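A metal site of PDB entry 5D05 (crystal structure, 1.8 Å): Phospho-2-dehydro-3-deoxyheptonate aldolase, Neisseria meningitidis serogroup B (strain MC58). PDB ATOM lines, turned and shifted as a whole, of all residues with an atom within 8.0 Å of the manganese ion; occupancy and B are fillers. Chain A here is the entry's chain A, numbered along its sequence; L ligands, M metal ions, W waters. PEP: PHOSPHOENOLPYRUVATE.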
ATOM      1  N   GLY A  61     -29.318  15.727  -4.001  1.00  0.00           N
ATOM      2  CA  GLY A  61     -29.747  14.372  -3.657  1.00  0.00           C
ATOM      3  C   GLY A  61     -30.091  14.283  -2.181  1.00  0.00           C
ATOM      4  O   GLY A  61     -30.190  15.302  -1.487  1.00  0.00           O
ATOM      5  N   PRO A  62     -30.285  13.057  -1.693  1.00  0.00           N
ATOM      6  CA  PRO A  62     -30.760  12.900  -0.305  1.00  0.00           C
ATOM      7  C   PRO A  62     -29.867  13.524   0.770  1.00  0.00           C
ATOM      8  O   PRO A  62     -28.648  13.648   0.585  1.00  0.00           O
ATOM      9  CB  PRO A  62     -30.783  11.377  -0.149  1.00  0.00           C
ATOM     10  CG  PRO A  62     -31.090  10.881  -1.534  1.00  0.00           C
ATOM     11  CD  PRO A  62     -30.255  11.773  -2.408  1.00  0.00           C
ATOM     12  N   CYS A  63     -30.475  13.921   1.895  1.00  0.00           N
ATOM     13  CA  CYS A  63     -29.686  14.316   3.054  1.00  0.00           C
ATOM     14  C   CYS A  63     -28.709  13.204   3.386  1.00  0.00           C
ATOM     15  O   CYS A  63     -27.476  13.426   3.543  1.00  0.00           O
ATOM     16  CB  CYS A  63     -30.594  14.583   4.259  1.00  0.00           C
ATOM     17  SG  CYS A  63     -29.660  14.909   5.756  1.00  0.00           S
ATOM     18  N   SER A  64     -29.248  12.011   3.516  1.00  0.00           N
ATOM     19  CA  SER A  64     -28.450  10.809   3.726  1.00  0.00           C
ATOM     20  C   SER A  64     -29.022   9.629   2.937  1.00  0.00           C
ATOM     21  O   SER A  64     -30.221   9.571   2.644  1.00  0.00           O
ATOM     22  CB  SER A  64     -28.350  10.457   5.230  1.00  0.00           C
ATOM     23  OG  SER A  64     -29.609  10.135   5.835  1.00  0.00           O
ATOM     24  N   ARG A  94     -25.666  14.007  -4.665  1.00  0.00           N
ATOM     25  CA  ARG A  94     -25.268  14.011  -3.240  1.00  0.00           C
ATOM     26  C   ARG A  94     -25.415  12.587  -2.699  1.00  0.00           C
ATOM     27  O   ARG A  94     -26.505  12.060  -2.625  1.00  0.00           O
ATOM     28  CB  ARG A  94     -26.160  14.983  -2.498  1.00  0.00           C
ATOM     29  CG  ARG A  94     -25.922  15.116  -1.015  1.00  0.00           C
ATOM     30  CD  ARG A  94     -26.882  16.102  -0.332  1.00  0.00           C
ATOM     31  NE  ARG A  94     -26.840  15.856   1.109  1.00  0.00           N
ATOM     32  CZ  ARG A  94     -26.193  16.585   2.032  1.00  0.00           C
ATOM     33  NH1 ARG A  94     -25.569  17.726   1.736  1.00  0.00           N
ATOM     34  NH2 ARG A  94     -26.221  16.185   3.286  1.00  0.00           N
ATOM     35  N   TYR A  96     -24.259  11.088   0.576  1.00  0.00           N
ATOM     36  CA  TYR A  96     -23.735  11.205   1.914  1.00  0.00           C
ATOM     37  C   TYR A  96     -24.304  10.069   2.717  1.00  0.00           C
ATOM     38  O   TYR A  96     -25.509   9.833   2.654  1.00  0.00           O
ATOM     39  CB  TYR A  96     -24.150  12.516   2.530  1.00  0.00           C
ATOM     40  CG  TYR A  96     -23.475  13.776   2.031  1.00  0.00           C
ATOM     41  CD1 TYR A  96     -23.088  13.923   0.706  1.00  0.00           C
ATOM     42  CD2 TYR A  96     -23.301  14.862   2.877  1.00  0.00           C
ATOM     43  CE1 TYR A  96     -22.510  15.099   0.256  1.00  0.00           C
ATOM     44  CE2 TYR A  96     -22.730  16.047   2.418  1.00  0.00           C
ATOM     45  CZ  TYR A  96     -22.341  16.153   1.093  1.00  0.00           C
ATOM     46  OH  TYR A  96     -21.807  17.331   0.633  1.00  0.00           O
ATOM     47  N   GLU A  98     -24.045   9.520   6.168  1.00  0.00           N
ATOM     48  CA  GLU A  98     -24.250   9.771   7.571  1.00  0.00           C
ATOM     49  C   GLU A  98     -24.580  11.269   7.729  1.00  0.00           C
ATOM     50  O   GLU A  98     -24.101  12.091   6.952  1.00  0.00           O
ATOM     51  CB  GLU A  98     -22.913   9.503   8.294  1.00  0.00           C
ATOM     52  CG  GLU A  98     -22.933   9.751   9.770  1.00  0.00           C
ATOM     53  CD  GLU A  98     -21.666   9.350  10.513  1.00  0.00           C
ATOM     54  OE1 GLU A  98     -20.760   8.730   9.947  1.00  0.00           O
ATOM     55  OE2 GLU A  98     -21.622   9.646  11.697  1.00  0.00           O
ATOM     56  N   LYS A  99     -25.363  11.615   8.723  1.00  0.00           N
ATOM     57  CA  LYS A  99     -25.413  13.010   9.166  1.00  0.00           C
ATOM     58  C   LYS A  99     -24.805  13.053  10.580  1.00  0.00           C
ATOM     59  O   LYS A  99     -25.251  12.309  11.454  1.00  0.00           O
ATOM     60  CB  LYS A  99     -26.844  13.570   9.238  1.00  0.00           C
ATOM     61  CG  LYS A  99     -26.838  15.058   9.555  1.00  0.00           C
ATOM     62  CD  LYS A  99     -28.189  15.753   9.773  1.00  0.00           C
ATOM     63  CE  LYS A  99     -27.937  17.264   9.717  1.00  0.00           C
ATOM     64  NZ  LYS A  99     -29.029  18.034  10.326  1.00  0.00           N
ATOM     65  N   PRO A 100     -23.819  13.936  10.798  1.00  0.00           N
ATOM     66  CA  PRO A 100     -23.247  14.022  12.158  1.00  0.00           C
ATOM     67  C   PRO A 100     -24.309  14.464  13.188  1.00  0.00           C
ATOM     68  O   PRO A 100     -25.269  15.178  12.822  1.00  0.00           O
ATOM     69  CB  PRO A 100     -22.160  15.081  12.027  1.00  0.00           C
ATOM     70  CG  PRO A 100     -21.843  15.157  10.571  1.00  0.00           C
ATOM     71  CD  PRO A 100     -23.127  14.836   9.845  1.00  0.00           C
ATOM     72  N   LYS A 188     -17.593  23.949   4.191  1.00  0.00           N
ATOM     73  CA  LYS A 188     -18.753  24.720   4.677  1.00  0.00           C
ATOM     74  C   LYS A 188     -18.324  25.768   5.703  1.00  0.00           C
ATOM     75  O   LYS A 188     -17.438  25.541   6.521  1.00  0.00           O
ATOM     76  CB  LYS A 188     -19.832  23.804   5.265  1.00  0.00           C
ATOM     77  CG  LYS A 188     -20.371  22.765   4.279  1.00  0.00           C
ATOM     78  CD  LYS A 188     -21.726  22.161   4.658  1.00  0.00           C
ATOM     79  CE  LYS A 188     -22.825  22.585   3.704  1.00  0.00           C
ATOM     80  NZ  LYS A 188     -24.158  22.014   4.053  1.00  0.00           N
ATOM     81  N   ASP A 267     -25.554  26.602  -0.428  1.00  0.00           N
ATOM     82  CA  ASP A 267     -26.479  25.528   0.013  1.00  0.00           C
ATOM     83  C   ASP A 267     -27.847  26.129   0.164  1.00  0.00           C
ATOM     84  O   ASP A 267     -28.024  27.123   0.893  1.00  0.00           O
ATOM     85  CB  ASP A 267     -25.968  24.952   1.361  1.00  0.00           C
ATOM     86  CG  ASP A 267     -26.710  23.703   1.829  1.00  0.00           C
ATOM     87  OD1 ASP A 267     -27.676  23.285   1.179  1.00  0.00           O
ATOM     88  OD2 ASP A 267     -26.283  23.137   2.880  1.00  0.00           O
ATOM     89  N   SER A 269     -30.294  24.428   1.450  1.00  0.00           N
ATOM     90  CA  SER A 269     -30.905  23.683   2.546  1.00  0.00           C
ATOM     91  C   SER A 269     -30.242  24.076   3.895  1.00  0.00           C
ATOM     92  O   SER A 269     -29.649  25.170   4.009  1.00  0.00           O
ATOM     93  CB  SER A 269     -30.801  22.183   2.270  1.00  0.00           C
ATOM     94  OG  SER A 269     -31.698  21.427   3.082  1.00  0.00           O
ATOM     95  N   HIS A 270     -30.394  23.229   4.907  1.00  0.00           N
ATOM     96  CA  HIS A 270     -29.763  23.432   6.215  1.00  0.00           C
ATOM     97  C   HIS A 270     -30.098  24.830   6.741  1.00  0.00           C
ATOM     98  O   HIS A 270     -31.292  25.221   6.644  1.00  0.00           O
ATOM     99  CB  HIS A 270     -28.286  23.084   6.148  1.00  0.00           C
ATOM    100  CG  HIS A 270     -28.082  21.672   5.691  1.00  0.00           C
ATOM    101  ND1 HIS A 270     -27.562  21.344   4.463  1.00  0.00           N
ATOM    102  CD2 HIS A 270     -28.447  20.502   6.275  1.00  0.00           C
ATOM    103  CE1 HIS A 270     -27.569  20.016   4.325  1.00  0.00           C
ATOM    104  NE2 HIS A 270     -28.113  19.488   5.416  1.00  0.00           N
ATOM    105  N   MET A 302     -26.172  23.631  -3.667  1.00  0.00           N
ATOM    106  CA  MET A 302     -26.484  22.338  -3.058  1.00  0.00           C
ATOM    107  C   MET A 302     -27.945  22.309  -2.675  1.00  0.00           C
ATOM    108  O   MET A 302     -28.518  23.315  -2.221  1.00  0.00           O
ATOM    109  CB  MET A 302     -25.561  22.107  -1.838  1.00  0.00           C
ATOM    110  CG  MET A 302     -25.786  20.839  -1.020  1.00  0.00           C
ATOM    111  SD  MET A 302     -24.612  20.721   0.374  1.00  0.00           S
ATOM    112  CE  MET A 302     -23.117  20.319  -0.510  1.00  0.00           C
ATOM    113  N   GLU A 304     -31.075  19.497  -1.070  1.00  0.00           N
ATOM    114  CA  GLU A 304     -31.489  18.254  -0.467  1.00  0.00           C
ATOM    115  C   GLU A 304     -32.822  17.804  -1.039  1.00  0.00           C
ATOM    116  O   GLU A 304     -33.866  18.431  -0.814  1.00  0.00           O
ATOM    117  CB  GLU A 304     -31.529  18.365   1.031  1.00  0.00           C
ATOM    118  CG  GLU A 304     -30.119  18.472   1.616  1.00  0.00           C
ATOM    119  CD  GLU A 304     -30.102  18.324   3.128  1.00  0.00           C
ATOM    120  OE1 GLU A 304     -30.854  19.042   3.845  1.00  0.00           O
ATOM    121  OE2 GLU A 304     -29.369  17.461   3.614  1.00  0.00           O
ATOM    122  N   SER A 321     -36.562  10.584   3.309  1.00  0.00           N
ATOM    123  CA  SER A 321     -35.450  10.799   4.241  1.00  0.00           C
ATOM    124  C   SER A 321     -35.795  10.425   5.678  1.00  0.00           C
ATOM    125  O   SER A 321     -36.901  10.694   6.138  1.00  0.00           O
ATOM    126  CB  SER A 321     -35.053  12.269   4.249  1.00  0.00           C
ATOM    127  OG  SER A 321     -33.914  12.493   5.082  1.00  0.00           O
ATOM    128  N   THR A 323     -33.263  11.491   7.843  1.00  0.00           N
ATOM    129  CA  THR A 323     -32.500  12.575   8.497  1.00  0.00           C
ATOM    130  C   THR A 323     -33.198  13.901   8.137  1.00  0.00           C
ATOM    131  O   THR A 323     -34.407  14.041   8.415  1.00  0.00           O
ATOM    132  CB  THR A 323     -30.991  12.470   8.178  1.00  0.00           C
ATOM    133  OG1 THR A 323     -30.782  12.389   6.757  1.00  0.00           O
ATOM    134  CG2 THR A 323     -30.398  11.199   8.808  1.00  0.00           C
ATOM    135  N   ASP A 324     -32.504  14.857   7.513  1.00  0.00           N
ATOM    136  CA  ASP A 324     -33.137  16.128   7.220  1.00  0.00           C
ATOM    137  C   ASP A 324     -34.228  15.947   6.162  1.00  0.00           C
ATOM    138  O   ASP A 324     -34.102  15.097   5.260  1.00  0.00           O
ATOM    139  CB  ASP A 324     -32.134  17.154   6.684  1.00  0.00           C
ATOM    140  CG  ASP A 324     -31.121  17.598   7.737  1.00  0.00           C
ATOM    141  OD1 ASP A 324     -31.436  17.622   8.927  1.00  0.00           O
ATOM    142  OD2 ASP A 324     -29.988  17.929   7.370  1.00  0.00           O
ATOM    143  N   ALA A 325     -35.277  16.764   6.265  1.00  0.00           N
ATOM    144  CA  ALA A 325     -36.362  16.761   5.282  1.00  0.00           C
ATOM    145  C   ALA A 325     -35.874  17.261   3.928  1.00  0.00           C
ATOM    146  O   ALA A 325     -35.054  18.183   3.853  1.00  0.00           O
ATOM    147  CB  ALA A 325     -37.547  17.575   5.762  1.00  0.00           C
ATOM    148  N   CYS A 326     -36.347  16.602   2.876  1.00  0.00           N
ATOM    149  CA  CYS A 326     -35.933  16.901   1.504  1.00  0.00           C
ATOM    150  C   CYS A 326     -37.120  17.282   0.648  1.00  0.00           C
ATOM    151  O   CYS A 326     -38.235  16.869   0.919  1.00  0.00           O
ATOM    152  CB  CYS A 326     -35.310  15.661   0.879  1.00  0.00           C
ATOM    153  SG  CYS A 326     -33.763  15.097   1.606  1.00  0.00           S
HETATM  154  C1  PEP L   1     -25.199  21.657   7.587  1.00  0.00           C
HETATM  155  O1  PEP L   1     -24.848  22.532   6.757  1.00  0.00           O
HETATM  156  O2' PEP L   1     -25.704  21.968   8.687  1.00  0.00           O
HETATM  157  C2  PEP L   1     -25.056  20.241   7.239  1.00  0.00           C
HETATM  158  C3  PEP L   1     -25.215  19.247   8.128  1.00  0.00           C
HETATM  159  O2  PEP L   1     -24.847  20.013   5.846  1.00  0.00           O
HETATM  160  P   PEP L   1     -24.019  18.794   5.172  1.00  0.00           P
HETATM  161  O1P PEP L   1     -24.000  19.261   3.734  1.00  0.00           O
HETATM  162  O2P PEP L   1     -22.643  18.788   5.841  1.00  0.00           O
HETATM  163  O3P PEP L   1     -24.785  17.542   5.463  1.00  0.00           O
HETATM  164 MN    MN M   1     -28.865  17.403   5.646  1.00  0.00          MN
HETATM  165  O   HOH W   1     -27.006  16.650   6.496  1.00  0.00           O
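The manganese ion is bound by OE2 of Glu 304 (2.1 Å), OD2 of Asp 324 (2.1 Å), water W1 (2.2 Å), NE2 of His 270 (2.2 Å) and SG of Cys 63 (2.6 Å). The manganese ion has five donor atoms within binding distance.
A ring nitrogen (ND1) of His 270 sits close to an oxygen (O2) of the ligand (3.3 Å). An oxygen (O3P) of the ligand lies within salt-bridge range of the guanidinium group (NH2) of Arg 94 (2.9 Å). NZ of Lys 188 lies within salt-bridge range of O1P of the ligand (2.8 Å).
The side-chain carboxylate of Glu 304 is in hydrogen-bond range of the side-chain hydroxyl of Ser 269 (2.6 Å). The side-chain carboxylate (OD1) of Asp 324 is in salt-bridge range of the side-chain amino group (NZ) of Lys 99 (2.8 Å). A ring nitrogen (ND1) of His 270 sits at hydrogen-bond distance from the side-chain amino group of Lys 188, at 3.5 Å. A ring nitrogen (ND1) of His 270 is in hydrogen-bond range of the side-chain carboxylate of Asp 267 (2.7 Å). O of Cys 63 is in hydrogen-bond range of NH2 of Arg 94, 3.0 Å away. N of Cys 63 lies within hydrogen-bond range of SG of Cys 326, at 3.5 Å. O of Pro 62 is in hydrogen-bond range of NE of Arg 94. The guanidinium group of Arg 94 is in hydrogen-bond range of the side-chain sulfur of Met 302 (3.4 Å).
Arg 94 touches the manganese ion. Five residues have an atom within 4 Å of the manganese ion: Cys 63, Arg 94, His 270, Glu 304 and Asp 324. The nearest printed residue that does not touch the manganese ion is Lys 99 (4.2 Å).
Water W1 bridges O3P of the ligand and NH2 of Arg 94.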
